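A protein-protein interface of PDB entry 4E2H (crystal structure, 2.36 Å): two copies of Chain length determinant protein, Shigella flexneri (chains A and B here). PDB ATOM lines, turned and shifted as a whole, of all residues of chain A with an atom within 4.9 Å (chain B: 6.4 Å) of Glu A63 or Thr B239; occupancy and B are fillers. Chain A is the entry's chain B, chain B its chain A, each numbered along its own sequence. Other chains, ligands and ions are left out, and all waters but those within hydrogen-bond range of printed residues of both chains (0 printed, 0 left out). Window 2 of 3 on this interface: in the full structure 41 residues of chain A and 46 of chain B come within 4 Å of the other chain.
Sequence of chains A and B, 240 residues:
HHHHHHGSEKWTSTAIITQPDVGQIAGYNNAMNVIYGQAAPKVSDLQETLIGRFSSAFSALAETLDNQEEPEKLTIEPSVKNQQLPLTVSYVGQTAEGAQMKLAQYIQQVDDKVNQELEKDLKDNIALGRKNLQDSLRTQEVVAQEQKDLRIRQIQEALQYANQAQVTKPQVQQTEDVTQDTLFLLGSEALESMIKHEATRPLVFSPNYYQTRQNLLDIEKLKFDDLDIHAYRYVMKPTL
The backbone carbonyl oxygen (O) of Ile B16 lies within hydrogen-bond range of the backbone NH (N) of Val B235, 2.7 Å away.
The backbone carbonyl oxygen (O) of Ile B16 lies within hydrogen-bond range of the backbone NH (N) of Met B236 (3.0 Å).
The side-chain hydroxyl (OG) of Ser B13 sits at hydrogen-bond distance from the backbone carbonyl oxygen (O) of Thr B239 (2.8 Å).
The side-chain hydroxyl of Thr B239 sits at hydrogen-bond distance from the backbone NH of Thr B14.
Among the printed residues, pairs that only touch across the chains: Ser A59 with Ile B16, Ala A60 with Ile B16, Ala A60 with Val B235, Ala A60 with Met B236, Glu A63 with Thr B14, Glu A63 with Met B236, Glu A63 with Thr B239 and Asn A67 with Leu B240.
Printed residues of chain B within 4 Å of Ser A59: Ile B16 (3.6 Å).
Printed residues of chain B within 4 Å of Ala A60: Ile B16, Val B235 and Met B236.
Ala A62 touches none of the printed residues of chain B.
Glu A63 touches just these residues of chain B: Thr B14 (3.6 Å), Met B236 (2.9 Å) and Thr B239 (3.8 Å).
Of the printed residues of chain A, Thr B14 touches Glu A63 (3.6 Å).
Of the printed residues of chain A, Ile B16 touches Ser A59 (3.6 Å) and Ala A60 (3.8 Å).
Ala B96 touches none of the printed residues of chain A.
Printed residues of chain A within 4 Å of Val B235: Ala A60 (3.9 Å).
Of chain A, only Glu A63 (3.8 Å) comes within 4 Å of Thr B239.
The nearest residue of chain B that does not touch Glu A63 is Ile B16 (4.05 Å).
Of the 18 printed residues of chain B, 6 touch a printed residue of chain A.
Hydrophobic or aromatic side chains of chain B that line the printed part of chain A: Ile B16, Val B235, Met B236 and Leu B240.
Along chain B the printed residues that touch a printed residue of chain A span positions 14 to 240.
Of the 9 printed residues of chain A, 4 touch a printed residue of chain B.
Printed residues of chain A that touch a printed residue of chain B: Ser A59, Ala A60, Glu A63 and Asn A67.
No position is printed for both chains.
Of the 8 pairs that touch across the chains among the printed residues, none has its exchanged pair printed and touching as well.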
ATOM      1  N   SER A  59      -4.724   6.897   7.789  1.00  0.00           N
ATOM      2  CA  SER A  59      -4.110   5.870   8.616  1.00  0.00           C
ATOM      3  C   SER A  59      -3.435   4.823   7.747  1.00  0.00           C
ATOM      4  O   SER A  59      -2.434   4.235   8.137  1.00  0.00           O
ATOM      5  CB  SER A  59      -5.169   5.177   9.482  1.00  0.00           C
ATOM      6  OG  SER A  59      -5.941   6.116  10.214  1.00  0.00           O
ATOM      7  N   ALA A  60      -4.006   4.556   6.579  1.00  0.00           N
ATOM      8  CA  ALA A  60      -3.415   3.572   5.694  1.00  0.00           C
ATOM      9  C   ALA A  60      -2.124   4.138   5.118  1.00  0.00           C
ATOM     10  O   ALA A  60      -1.126   3.430   5.019  1.00  0.00           O
ATOM     11  CB  ALA A  60      -4.377   3.187   4.599  1.00  0.00           C
ATOM     12  N   LEU A  61      -2.135   5.420   4.764  1.00  0.00           N
ATOM     13  CA  LEU A  61      -0.956   6.045   4.171  1.00  0.00           C
ATOM     14  C   LEU A  61       0.204   6.015   5.163  1.00  0.00           C
ATOM     15  O   LEU A  61       1.349   5.732   4.790  1.00  0.00           O
ATOM     16  CB  LEU A  61      -1.255   7.476   3.766  1.00  0.00           C
ATOM     17  CG  LEU A  61      -0.143   8.221   3.035  1.00  0.00           C
ATOM     18  CD1 LEU A  61       0.442   7.360   1.917  1.00  0.00           C
ATOM     19  CD2 LEU A  61      -0.659   9.572   2.495  1.00  0.00           C
ATOM     20  N   ALA A  62      -0.105   6.278   6.433  1.00  0.00           N
ATOM     21  CA  ALA A  62       0.907   6.280   7.482  1.00  0.00           C
ATOM     22  C   ALA A  62       1.385   4.870   7.844  1.00  0.00           C
ATOM     23  O   ALA A  62       2.585   4.644   7.948  1.00  0.00           O
ATOM     24  CB  ALA A  62       0.421   7.050   8.727  1.00  0.00           C
ATOM     25  N   GLU A  63       0.461   3.928   8.031  1.00  0.00           N
ATOM     26  CA  GLU A  63       0.821   2.518   8.168  1.00  0.00           C
ATOM     27  C   GLU A  63       1.931   2.150   7.183  1.00  0.00           C
ATOM     28  O   GLU A  63       2.937   1.553   7.570  1.00  0.00           O
ATOM     29  CB  GLU A  63      -0.407   1.614   7.932  1.00  0.00           C
ATOM     30  CG  GLU A  63      -0.159   0.336   7.076  1.00  0.00           C
ATOM     31  CD  GLU A  63      -1.431  -0.182   6.311  1.00  0.00           C
ATOM     32  OE1 GLU A  63      -2.020  -1.186   6.741  1.00  0.00           O
ATOM     33  OE2 GLU A  63      -1.821   0.385   5.275  1.00  0.00           O
ATOM     34  N   THR A  64       1.752   2.503   5.910  1.00  0.00           N
ATOM     35  CA  THR A  64       2.676   2.035   4.878  1.00  0.00           C
ATOM     36  C   THR A  64       3.959   2.850   4.809  1.00  0.00           C
ATOM     37  O   THR A  64       5.003   2.333   4.424  1.00  0.00           O
ATOM     38  CB  THR A  64       2.026   1.964   3.463  1.00  0.00           C
ATOM     39  OG1 THR A  64       1.863   3.283   2.929  1.00  0.00           O
ATOM     40  CG2 THR A  64       0.672   1.264   3.515  1.00  0.00           C
ATOM     41  N   LEU A  65       3.884   4.128   5.165  1.00  0.00           N
ATOM     42  CA  LEU A  65       5.078   4.961   5.171  1.00  0.00           C
ATOM     43  C   LEU A  65       6.087   4.453   6.195  1.00  0.00           C
ATOM     44  O   LEU A  65       7.291   4.603   6.017  1.00  0.00           O
ATOM     45  CB  LEU A  65       4.723   6.424   5.424  1.00  0.00           C
ATOM     46  CG  LEU A  65       4.200   7.166   4.190  1.00  0.00           C
ATOM     47  CD1 LEU A  65       3.801   8.587   4.518  1.00  0.00           C
ATOM     48  CD2 LEU A  65       5.252   7.157   3.098  1.00  0.00           C
ATOM     49  N   ASP A  66       5.579   3.840   7.259  1.00  0.00           N
ATOM     50  CA  ASP A  66       6.401   3.316   8.345  1.00  0.00           C
ATOM     51  C   ASP A  66       7.024   1.973   7.942  1.00  0.00           C
ATOM     52  O   ASP A  66       7.824   1.376   8.679  1.00  0.00           O
ATOM     53  CB  ASP A  66       5.521   3.143   9.587  1.00  0.00           C
ATOM     54  CG  ASP A  66       6.323   2.912  10.855  1.00  0.00           C
ATOM     55  OD1 ASP A  66       6.892   3.908  11.374  1.00  0.00           O
ATOM     56  OD2 ASP A  66       6.369   1.751  11.344  1.00  0.00           O
ATOM     57  N   ASN A  67       6.663   1.504   6.756  1.00  0.00           N
ATOM     58  CA  ASN A  67       7.046   0.169   6.336  1.00  0.00           C
ATOM     59  C   ASN A  67       7.856   0.198   5.039  1.00  0.00           C
ATOM     60  O   ASN A  67       7.463  -0.396   4.030  1.00  0.00           O
ATOM     61  CB  ASN A  67       5.793  -0.711   6.207  1.00  0.00           C
ATOM     62  CG  ASN A  67       6.109  -2.193   6.134  1.00  0.00           C
ATOM     63  OD1 ASN A  67       5.467  -3.013   6.801  1.00  0.00           O
ATOM     64  ND2 ASN A  67       7.086  -2.547   5.310  1.00  0.00           N
ATOM     65  N   THR B  12       5.387  -9.839  11.803  1.00  0.00           N
ATOM     66  CA  THR B  12       4.155  -9.093  12.112  1.00  0.00           C
ATOM     67  C   THR B  12       3.513  -8.383  10.920  1.00  0.00           C
ATOM     68  O   THR B  12       4.171  -7.609  10.202  1.00  0.00           O
ATOM     69  CB  THR B  12       4.342  -8.061  13.247  1.00  0.00           C
ATOM     70  OG1 THR B  12       4.212  -8.740  14.497  1.00  0.00           O
ATOM     71  CG2 THR B  12       3.261  -7.005  13.186  1.00  0.00           C
ATOM     72  N   SER B  13       2.224  -8.657  10.722  1.00  0.00           N
ATOM     73  CA  SER B  13       1.459  -8.073   9.618  1.00  0.00           C
ATOM     74  C   SER B  13       0.280  -7.268  10.144  1.00  0.00           C
ATOM     75  O   SER B  13      -0.388  -7.696  11.103  1.00  0.00           O
ATOM     76  CB  SER B  13       0.944  -9.168   8.657  1.00  0.00           C
ATOM     77  OG  SER B  13       0.413  -8.573   7.481  1.00  0.00           O
ATOM     78  N   THR B  14       0.024  -6.126   9.500  1.00  0.00           N
ATOM     79  CA  THR B  14      -1.107  -5.267   9.851  1.00  0.00           C
ATOM     80  C   THR B  14      -1.995  -4.949   8.642  1.00  0.00           C
ATOM     81  O   THR B  14      -1.497  -4.674   7.537  1.00  0.00           O
ATOM     82  CB  THR B  14      -0.657  -3.906  10.463  1.00  0.00           C
ATOM     83  OG1 THR B  14       0.363  -4.118  11.450  1.00  0.00           O
ATOM     84  CG2 THR B  14      -1.849  -3.182  11.096  1.00  0.00           C
ATOM     85  N   ALA B  15      -3.312  -4.984   8.866  1.00  0.00           N
ATOM     86  CA  ALA B  15      -4.302  -4.445   7.930  1.00  0.00           C
ATOM     87  C   ALA B  15      -5.228  -3.481   8.684  1.00  0.00           C
ATOM     88  O   ALA B  15      -5.351  -3.569   9.921  1.00  0.00           O
ATOM     89  CB  ALA B  15      -5.110  -5.573   7.298  1.00  0.00           C
ATOM     90  N   ILE B  16      -5.863  -2.566   7.949  1.00  0.00           N
ATOM     91  CA  ILE B  16      -6.901  -1.687   8.499  1.00  0.00           C
ATOM     92  C   ILE B  16      -8.253  -1.947   7.806  1.00  0.00           C
ATOM     93  O   ILE B  16      -8.375  -1.819   6.585  1.00  0.00           O
ATOM     94  CB  ILE B  16      -6.535  -0.192   8.320  1.00  0.00           C
ATOM     95  CG1 ILE B  16      -5.270   0.149   9.102  1.00  0.00           C
ATOM     96  CG2 ILE B  16      -7.685   0.713   8.750  1.00  0.00           C
ATOM     97  CD1 ILE B  16      -4.545   1.389   8.576  1.00  0.00           C
ATOM     98  N   THR B  88      -7.774  -1.464  13.298  1.00  0.00           N
ATOM     99  CA  THR B  88      -6.488  -1.973  12.897  1.00  0.00           C
ATOM    100  C   THR B  88      -6.308  -3.375  13.476  1.00  0.00           C
ATOM    101  O   THR B  88      -6.557  -3.615  14.669  1.00  0.00           O
ATOM    102  CB  THR B  88      -5.369  -1.018  13.324  1.00  0.00           C
ATOM    103  OG1 THR B  88      -4.283  -1.094  12.390  1.00  0.00           O
ATOM    104  CG2 THR B  88      -4.882  -1.346  14.724  1.00  0.00           C
ATOM    105  N   ALA B  96       7.585 -12.515   6.388  1.00  0.00           N
ATOM    106  CA  ALA B  96       6.786 -11.464   5.759  1.00  0.00           C
ATOM    107  C   ALA B  96       5.668 -12.119   4.964  1.00  0.00           C
ATOM    108  O   ALA B  96       4.483 -11.846   5.189  1.00  0.00           O
ATOM    109  CB  ALA B  96       7.634 -10.598   4.852  1.00  0.00           C
ATOM    110  N   GLU B  97       6.046 -12.981   4.027  1.00  0.00           N
ATOM    111  CA  GLU B  97       5.064 -13.785   3.323  1.00  0.00           C
ATOM    112  C   GLU B  97       4.248 -14.575   4.359  1.00  0.00           C
ATOM    113  O   GLU B  97       3.021 -14.657   4.261  1.00  0.00           O
ATOM    114  CB  GLU B  97       5.752 -14.715   2.317  1.00  0.00           C
ATOM    115  N   ALA B  99       3.436 -14.072   7.728  1.00  0.00           N
ATOM    116  CA  ALA B  99       2.475 -13.427   8.623  1.00  0.00           C
ATOM    117  C   ALA B  99       1.392 -12.654   7.874  1.00  0.00           C
ATOM    118  O   ALA B  99       0.291 -12.464   8.399  1.00  0.00           O
ATOM    119  CB  ALA B  99       3.192 -12.529   9.669  1.00  0.00           C
ATOM    120  N   GLN B 100       1.703 -12.236   6.646  1.00  0.00           N
ATOM    121  CA  GLN B 100       0.740 -11.575   5.749  1.00  0.00           C
ATOM    122  C   GLN B 100      -0.470 -12.471   5.443  1.00  0.00           C
ATOM    123  O   GLN B 100      -1.580 -12.226   5.921  1.00  0.00           O
ATOM    124  CB  GLN B 100       1.430 -11.173   4.439  1.00  0.00           C
ATOM    125  CG  GLN B 100       0.749 -10.070   3.660  1.00  0.00           C
ATOM    126  CD  GLN B 100       1.422  -9.795   2.319  1.00  0.00           C
ATOM    127  OE1 GLN B 100       2.037 -10.689   1.719  1.00  0.00           O
ATOM    128  NE2 GLN B 100       1.307  -8.551   1.836  1.00  0.00           N
ATOM    129  N   MET B 101      -0.256 -13.509   4.643  1.00  0.00           N
ATOM    130  CA  MET B 101      -1.343 -14.420   4.299  1.00  0.00           C
ATOM    131  C   MET B 101      -1.959 -15.098   5.527  1.00  0.00           C
ATOM    132  O   MET B 101      -3.139 -15.457   5.527  1.00  0.00           O
ATOM    133  CB  MET B 101      -0.882 -15.477   3.297  1.00  0.00           C
ATOM    134  CG  MET B 101       0.356 -16.242   3.748  1.00  0.00           C
ATOM    135  SD  MET B 101       0.727 -17.834   2.669  1.00  0.00           S
ATOM    136  CE  MET B 101      -0.349 -19.133   3.652  1.00  0.00           C
ATOM    137  N   LEU B 103      -2.579 -13.601   8.163  1.00  0.00           N
ATOM    138  CA  LEU B 103      -3.557 -12.597   8.579  1.00  0.00           C
ATOM    139  C   LEU B 103      -4.728 -12.531   7.600  1.00  0.00           C
ATOM    140  O   LEU B 103      -5.889 -12.433   8.022  1.00  0.00           O
ATOM    141  CB  LEU B 103      -2.914 -11.210   8.697  1.00  0.00           C
ATOM    142  CG  LEU B 103      -3.883 -10.125   9.169  1.00  0.00           C
ATOM    143  CD1 LEU B 103      -4.319 -10.401  10.609  1.00  0.00           C
ATOM    144  CD2 LEU B 103      -3.283  -8.740   9.044  1.00  0.00           C
ATOM    145  N   VAL B 235      -9.441  -1.169   4.140  1.00  0.00           N
ATOM    146  CA  VAL B 235      -8.874   0.145   3.868  1.00  0.00           C
ATOM    147  C   VAL B 235      -7.409  -0.053   3.504  1.00  0.00           C
ATOM    148  O   VAL B 235      -6.849   0.672   2.686  1.00  0.00           O
ATOM    149  CB  VAL B 235      -8.959   1.049   5.095  1.00  0.00           C
ATOM    150  CG1 VAL B 235      -8.129   2.306   4.886  1.00  0.00           C
ATOM    151  CG2 VAL B 235     -10.399   1.390   5.385  1.00  0.00           C
ATOM    152  N   MET B 236      -6.796  -1.039   4.150  1.00  0.00           N
ATOM    153  CA  MET B 236      -5.431  -1.434   3.855  1.00  0.00           C
ATOM    154  C   MET B 236      -5.327  -2.952   3.969  1.00  0.00           C
ATOM    155  O   MET B 236      -5.522  -3.534   5.050  1.00  0.00           O
ATOM    156  CB  MET B 236      -4.444  -0.749   4.811  1.00  0.00           C
ATOM    157  N   LYS B 237      -5.047  -3.593   2.841  1.00  0.00           N
ATOM    158  CA  LYS B 237      -4.786  -5.020   2.831  1.00  0.00           C
ATOM    159  C   LYS B 237      -3.476  -5.302   3.598  1.00  0.00           C
ATOM    160  O   LYS B 237      -2.525  -4.493   3.533  1.00  0.00           O
ATOM    161  CB  LYS B 237      -4.715  -5.521   1.384  1.00  0.00           C
ATOM    162  N   PRO B 238      -3.413  -6.450   4.319  1.00  0.00           N
ATOM    163  CA  PRO B 238      -2.279  -6.774   5.205  1.00  0.00           C
ATOM    164  C   PRO B 238      -0.915  -6.607   4.548  1.00  0.00           C
ATOM    165  O   PRO B 238      -0.788  -6.643   3.319  1.00  0.00           O
ATOM    166  CB  PRO B 238      -2.508  -8.239   5.595  1.00  0.00           C
ATOM    167  CG  PRO B 238      -3.621  -8.735   4.710  1.00  0.00           C
ATOM    168  CD  PRO B 238      -4.419  -7.528   4.297  1.00  0.00           C
ATOM    169  N   THR B 239       0.097  -6.443   5.394  1.00  0.00           N
ATOM    170  CA  THR B 239       1.377  -5.892   4.979  1.00  0.00           C
ATOM    171  C   THR B 239       2.517  -6.897   4.978  1.00  0.00           C
ATOM    172  O   THR B 239       2.376  -7.992   5.528  1.00  0.00           O
ATOM    173  CB  THR B 239       1.771  -4.728   5.920  1.00  0.00           C
ATOM    174  OG1 THR B 239       1.674  -5.154   7.294  1.00  0.00           O
ATOM    175  CG2 THR B 239       0.849  -3.515   5.684  1.00  0.00           C
ATOM    176  N   LEU B 240       3.640  -6.505   4.359  1.00  0.00           N
ATOM    177  CA  LEU B 240       4.923  -7.232   4.435  1.00  0.00           C
ATOM    178  C   LEU B 240       5.866  -6.652   5.527  1.00  0.00           C
ATOM    179  O   LEU B 240       6.138  -7.280   6.568  1.00  0.00           O
ATOM    180  CB  LEU B 240       5.612  -7.209   3.055  1.00  0.00           C
ATOM    181  CG  LEU B 240       5.927  -5.803   2.500  1.00  0.00           C
ATOM    182  CD1 LEU B 240       7.139  -5.168   3.204  1.00  0.00           C
ATOM    183  CD2 LEU B 240       6.134  -5.791   0.984  1.00  0.00           C
